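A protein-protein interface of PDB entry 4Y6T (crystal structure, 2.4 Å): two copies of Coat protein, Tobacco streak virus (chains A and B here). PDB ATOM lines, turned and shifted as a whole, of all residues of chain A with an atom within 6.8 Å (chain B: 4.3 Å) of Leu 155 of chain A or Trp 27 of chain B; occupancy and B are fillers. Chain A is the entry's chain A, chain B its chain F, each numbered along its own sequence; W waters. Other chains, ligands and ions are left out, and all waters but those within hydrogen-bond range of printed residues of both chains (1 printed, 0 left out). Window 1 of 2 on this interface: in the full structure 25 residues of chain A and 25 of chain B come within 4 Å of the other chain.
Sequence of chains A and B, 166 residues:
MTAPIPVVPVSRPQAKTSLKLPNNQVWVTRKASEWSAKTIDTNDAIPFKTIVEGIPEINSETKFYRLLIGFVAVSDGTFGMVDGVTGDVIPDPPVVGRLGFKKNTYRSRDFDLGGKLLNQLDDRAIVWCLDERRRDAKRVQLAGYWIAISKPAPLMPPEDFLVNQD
Water W1 lies within hydrogen-bond range of O of Leu 155 of chain A (3.0 Å) and N of Trp 27 of chain B (3.0 Å).
Leu 155 of chain A touches just one residue of chain B: Trp 27.
Of the printed residues of chain B, Met 156 of chain A touches Leu 19 (3.6 Å), Trp 27 (3.98 Å) and Trp 146 (3.5 Å).
Of the printed residues of chain B, Pro 157 of chain A touches Leu 19 (3.6 Å), Trp 27 (3.5 Å) and Trp 146 (3.7 Å).
Arg 66 of chain B touches none of the printed residues of chain A.
Printed residues of chain A within 4 Å of Trp 146 of chain B: Met 156 and Pro 157.
Ala 148 of chain B touches none of the printed residues of chain A.
The nearest printed residue of chain B that does not touch Leu 155 of chain A is Trp 146 of chain B (4.3 Å).
The nearest residue of chain A that does not touch Trp 27 of chain B is Pro 154 of chain A (6.4 Å).
Of the 10 printed residues of chain B, 3 touch a printed residue of chain A.
Hydrophobic or aromatic side chains of chain A that line the printed part of chain B: Leu 155, Met 156 and Pro 157.
CD1 of Trp 27 of chain B touches O of Leu 155 of chain A, at 3.4 Å.
Leu 19 of chain B touches Met 156 of chain A.
Trp 27 of chain B touches Met 156 of chain A.
CH2 of Trp 146 of chain B touches O of Met 156 of chain A, at 3.5 Å.
CD1 of Leu 19 of chain B touches O of Pro 157 of chain A (3.6 Å).
Pro 157 of chain A touches Trp 27 of chain B (CD to NE1, 3.5 Å).
Trp 146 of chain B touches Pro 157 of chain A (CZ3 to N, 3.7 Å).
N of Leu 68 of chain B sits at hydrogen-bond distance from O of Trp 146 of chain B, 2.8 Å away.
The backbone carbonyl oxygen (O) of Leu 19 of chain B is in hydrogen-bond range of the indole nitrogen (NE1) of Trp 27 of chain B, at 2.9 Å.
No position is printed for both chains.
Of the 7 pairs that touch across the chains among the printed residues, none has its exchanged pair printed and touching as well.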
ATOM      1  N   PRO A 152      -3.572  13.762  23.189  1.00  0.00           N
ATOM      2  CA  PRO A 152      -2.581  12.861  22.624  1.00  0.00           C
ATOM      3  C   PRO A 152      -2.799  12.656  21.173  1.00  0.00           C
ATOM      4  O   PRO A 152      -3.813  13.082  20.554  1.00  0.00           O
ATOM      5  CB  PRO A 152      -2.911  11.512  23.241  1.00  0.00           C
ATOM      6  CG  PRO A 152      -4.383  11.605  23.465  1.00  0.00           C
ATOM      7  CD  PRO A 152      -4.756  13.059  23.668  1.00  0.00           C
ATOM      8  N   ALA A 153      -1.787  12.003  20.649  1.00  0.00           N
ATOM      9  CA  ALA A 153      -1.787  11.585  19.261  1.00  0.00           C
ATOM     10  C   ALA A 153      -2.968  10.657  19.049  1.00  0.00           C
ATOM     11  O   ALA A 153      -3.246   9.791  19.881  1.00  0.00           O
ATOM     12  CB  ALA A 153      -0.476  10.889  18.942  1.00  0.00           C
ATOM     13  N   PRO A 154      -3.669  10.815  17.953  1.00  0.00           N
ATOM     14  CA  PRO A 154      -4.761   9.858  17.685  1.00  0.00           C
ATOM     15  C   PRO A 154      -4.275   8.377  17.579  1.00  0.00           C
ATOM     16  O   PRO A 154      -3.159   8.139  17.170  1.00  0.00           O
ATOM     17  CB  PRO A 154      -5.300  10.324  16.337  1.00  0.00           C
ATOM     18  CG  PRO A 154      -4.755  11.701  16.124  1.00  0.00           C
ATOM     19  CD  PRO A 154      -3.424  11.700  16.810  1.00  0.00           C
ATOM     20  N   LEU A 155      -5.102   7.421  17.991  1.00  0.00           N
ATOM     21  CA  LEU A 155      -4.851   6.002  17.746  1.00  0.00           C
ATOM     22  C   LEU A 155      -4.871   5.656  16.257  1.00  0.00           C
ATOM     23  O   LEU A 155      -5.699   6.159  15.490  1.00  0.00           O
ATOM     24  CB  LEU A 155      -5.901   5.149  18.417  1.00  0.00           C
ATOM     25  CG  LEU A 155      -5.758   4.875  19.874  1.00  0.00           C
ATOM     26  CD1 LEU A 155      -6.573   3.659  20.291  1.00  0.00           C
ATOM     27  CD2 LEU A 155      -4.307   4.682  20.267  1.00  0.00           C
ATOM     28  N   MET A 156      -3.929   4.821  15.860  1.00  0.00           N
ATOM     29  CA  MET A 156      -3.820   4.325  14.483  1.00  0.00           C
ATOM     30  C   MET A 156      -3.550   2.844  14.537  1.00  0.00           C
ATOM     31  O   MET A 156      -2.722   2.381  15.337  1.00  0.00           O
ATOM     32  CB  MET A 156      -2.655   4.971  13.761  1.00  0.00           C
ATOM     33  CG  MET A 156      -2.874   6.438  13.527  1.00  0.00           C
ATOM     34  SD  MET A 156      -4.199   6.717  12.367  1.00  0.00           S
ATOM     35  CE  MET A 156      -3.226   6.646  10.852  1.00  0.00           C
ATOM     36  N   PRO A 157      -4.238   2.075  13.681  1.00  0.00           N
ATOM     37  CA  PRO A 157      -3.831   0.675  13.554  1.00  0.00           C
ATOM     38  C   PRO A 157      -2.398   0.569  13.015  1.00  0.00           C
ATOM     39  O   PRO A 157      -1.941   1.485  12.321  1.00  0.00           O
ATOM     40  CB  PRO A 157      -4.806   0.121  12.503  1.00  0.00           C
ATOM     41  CG  PRO A 157      -5.852   1.160  12.320  1.00  0.00           C
ATOM     42  CD  PRO A 157      -5.208   2.455  12.653  1.00  0.00           C
ATOM     43  N   LEU A 162      -3.412  -4.257   7.185  1.00  0.00           N
ATOM     44  CA  LEU A 162      -4.210  -4.716   6.075  1.00  0.00           C
ATOM     45  C   LEU A 162      -3.434  -5.424   4.971  1.00  0.00           C
ATOM     46  O   LEU A 162      -3.849  -5.422   3.813  1.00  0.00           O
ATOM     47  CB  LEU A 162      -4.972  -3.531   5.498  1.00  0.00           C
ATOM     48  CG  LEU A 162      -6.111  -3.062   6.366  1.00  0.00           C
ATOM     49  CD1 LEU A 162      -6.771  -1.840   5.739  1.00  0.00           C
ATOM     50  CD2 LEU A 162      -7.144  -4.166   6.569  1.00  0.00           C
ATOM     51  N   LEU B  19      -4.382   4.837   6.714  1.00  0.00           N
ATOM     52  CA  LEU B  19      -5.413   4.614   7.719  1.00  0.00           C
ATOM     53  C   LEU B  19      -5.862   5.949   8.372  1.00  0.00           C
ATOM     54  O   LEU B  19      -6.501   5.932   9.408  1.00  0.00           O
ATOM     55  CB  LEU B  19      -4.729   3.689   8.699  1.00  0.00           C
ATOM     56  CG  LEU B  19      -4.456   2.267   8.158  1.00  0.00           C
ATOM     57  CD1 LEU B  19      -3.534   1.482   9.091  1.00  0.00           C
ATOM     58  CD2 LEU B  19      -5.753   1.506   7.925  1.00  0.00           C
ATOM     59  N   LEU B  21      -8.207   9.079   9.022  1.00  0.00           N
ATOM     60  CA  LEU B  21      -9.648   9.181   8.926  1.00  0.00           C
ATOM     61  C   LEU B  21     -10.124  10.619   8.732  1.00  0.00           C
ATOM     62  O   LEU B  21      -9.414  11.566   9.028  1.00  0.00           O
ATOM     63  CB  LEU B  21     -10.301   8.630  10.192  1.00  0.00           C
ATOM     64  CG  LEU B  21     -10.058   7.135  10.439  1.00  0.00           C
ATOM     65  CD1 LEU B  21     -10.402   6.675  11.845  1.00  0.00           C
ATOM     66  CD2 LEU B  21     -10.811   6.296   9.421  1.00  0.00           C
ATOM     67  N   VAL B  26     -12.651   8.639  14.771  1.00  0.00           N
ATOM     68  CA  VAL B  26     -11.482   8.060  15.422  1.00  0.00           C
ATOM     69  C   VAL B  26     -11.496   6.561  15.309  1.00  0.00           C
ATOM     70  O   VAL B  26     -12.563   5.932  15.152  1.00  0.00           O
ATOM     71  CB  VAL B  26     -11.425   8.361  16.928  1.00  0.00           C
ATOM     72  CG1 VAL B  26     -11.227   9.859  17.184  1.00  0.00           C
ATOM     73  CG2 VAL B  26     -12.686   7.848  17.626  1.00  0.00           C
ATOM     74  N   TRP B  27     -10.288   6.003  15.412  1.00  0.00           N
ATOM     75  CA  TRP B  27     -10.114   4.575  15.611  1.00  0.00           C
ATOM     76  C   TRP B  27     -10.200   4.215  17.077  1.00  0.00           C
ATOM     77  O   TRP B  27      -9.657   4.897  17.924  1.00  0.00           O
ATOM     78  CB  TRP B  27      -8.702   4.149  15.153  1.00  0.00           C
ATOM     79  CG  TRP B  27      -8.498   4.143  13.707  1.00  0.00           C
ATOM     80  CD1 TRP B  27      -7.727   4.992  13.002  1.00  0.00           C
ATOM     81  CD2 TRP B  27      -9.102   3.253  12.768  1.00  0.00           C
ATOM     82  NE1 TRP B  27      -7.795   4.677  11.684  1.00  0.00           N
ATOM     83  CE2 TRP B  27      -8.642   3.614  11.515  1.00  0.00           C
ATOM     84  CE3 TRP B  27      -9.947   2.141  12.889  1.00  0.00           C
ATOM     85  CZ2 TRP B  27      -8.990   2.910  10.364  1.00  0.00           C
ATOM     86  CZ3 TRP B  27     -10.314   1.452  11.771  1.00  0.00           C
ATOM     87  CH2 TRP B  27      -9.848   1.835  10.514  1.00  0.00           C
ATOM     88  N   VAL B  28     -10.816   3.088  17.359  1.00  0.00           N
ATOM     89  CA  VAL B  28     -10.710   2.451  18.631  1.00  0.00           C
ATOM     90  C   VAL B  28     -10.391   0.986  18.424  1.00  0.00           C
ATOM     91  O   VAL B  28     -10.633   0.445  17.337  1.00  0.00           O
ATOM     92  CB  VAL B  28     -11.985   2.556  19.436  1.00  0.00           C
ATOM     93  CG1 VAL B  28     -12.213   4.001  19.800  1.00  0.00           C
ATOM     94  CG2 VAL B  28     -13.189   1.982  18.683  1.00  0.00           C
ATOM     95  N   ARG B  66     -15.892   1.565   9.724  1.00  0.00           N
ATOM     96  CA  ARG B  66     -15.026   0.502   9.289  1.00  0.00           C
ATOM     97  C   ARG B  66     -14.713  -0.432  10.411  1.00  0.00           C
ATOM     98  O   ARG B  66     -14.514   0.018  11.527  1.00  0.00           O
ATOM     99  CB  ARG B  66     -13.736   1.076   8.762  1.00  0.00           C
ATOM    100  CG  ARG B  66     -13.942   1.947   7.533  1.00  0.00           C
ATOM    101  CD  ARG B  66     -12.701   2.762   7.188  1.00  0.00           C
ATOM    102  NE  ARG B  66     -11.608   1.903   6.775  1.00  0.00           N
ATOM    103  CZ  ARG B  66     -10.366   2.332   6.549  1.00  0.00           C
ATOM    104  NH1 ARG B  66     -10.040   3.606   6.716  1.00  0.00           N
ATOM    105  NH2 ARG B  66      -9.436   1.477   6.162  1.00  0.00           N
ATOM    106  N   LEU B  68     -11.885  -3.423  10.914  1.00  0.00           N
ATOM    107  CA  LEU B  68     -10.753  -4.148  10.424  1.00  0.00           C
ATOM    108  C   LEU B  68     -10.505  -5.360  11.299  1.00  0.00           C
ATOM    109  O   LEU B  68     -10.453  -5.252  12.515  1.00  0.00           O
ATOM    110  CB  LEU B  68      -9.480  -3.347  10.453  1.00  0.00           C
ATOM    111  CG  LEU B  68      -9.519  -1.913   9.988  1.00  0.00           C
ATOM    112  CD1 LEU B  68      -8.110  -1.321  10.019  1.00  0.00           C
ATOM    113  CD2 LEU B  68     -10.103  -1.776   8.617  1.00  0.00           C
ATOM    114  N   TRP B 146     -10.105  -3.377  15.002  1.00  0.00           N
ATOM    115  CA  TRP B 146     -10.046  -1.934  14.840  1.00  0.00           C
ATOM    116  C   TRP B 146     -11.374  -1.420  14.261  1.00  0.00           C
ATOM    117  O   TRP B 146     -11.914  -1.988  13.329  1.00  0.00           O
ATOM    118  CB  TRP B 146      -8.872  -1.559  13.957  1.00  0.00           C
ATOM    119  CG  TRP B 146      -7.617  -1.712  14.684  1.00  0.00           C
ATOM    120  CD1 TRP B 146      -6.865  -2.836  14.754  1.00  0.00           C
ATOM    121  CD2 TRP B 146      -6.964  -0.745  15.471  1.00  0.00           C
ATOM    122  NE1 TRP B 146      -5.774  -2.636  15.543  1.00  0.00           N
ATOM    123  CE2 TRP B 146      -5.814  -1.358  16.014  1.00  0.00           C
ATOM    124  CE3 TRP B 146      -7.231   0.584  15.789  1.00  0.00           C
ATOM    125  CZ2 TRP B 146      -4.931  -0.688  16.866  1.00  0.00           C
ATOM    126  CZ3 TRP B 146      -6.344   1.261  16.609  1.00  0.00           C
ATOM    127  CH2 TRP B 146      -5.206   0.615  17.149  1.00  0.00           C
ATOM    128  N   ILE B 147     -11.884  -0.350  14.831  1.00  0.00           N
ATOM    129  CA  ILE B 147     -13.169   0.187  14.442  1.00  0.00           C
ATOM    130  C   ILE B 147     -13.102   1.667  14.258  1.00  0.00           C
ATOM    131  O   ILE B 147     -12.661   2.387  15.138  1.00  0.00           O
ATOM    132  CB  ILE B 147     -14.195  -0.102  15.488  1.00  0.00           C
ATOM    133  CG1 ILE B 147     -13.967  -1.509  16.007  1.00  0.00           C
ATOM    134  CG2 ILE B 147     -15.582   0.072  14.881  1.00  0.00           C
ATOM    135  CD1 ILE B 147     -14.927  -1.946  17.061  1.00  0.00           C
ATOM    136  N   ALA B 148     -13.468   2.138  13.071  1.00  0.00           N
ATOM    137  CA  ALA B 148     -13.515   3.570  12.811  1.00  0.00           C
ATOM    138  C   ALA B 148     -14.902   4.032  13.172  1.00  0.00           C
ATOM    139  O   ALA B 148     -15.864   3.513  12.648  1.00  0.00           O
ATOM    140  CB  ALA B 148     -13.254   3.864  11.370  1.00  0.00           C
HETATM  141  O   HOH W   1      -8.041   7.973  15.893  1.00  0.00           O
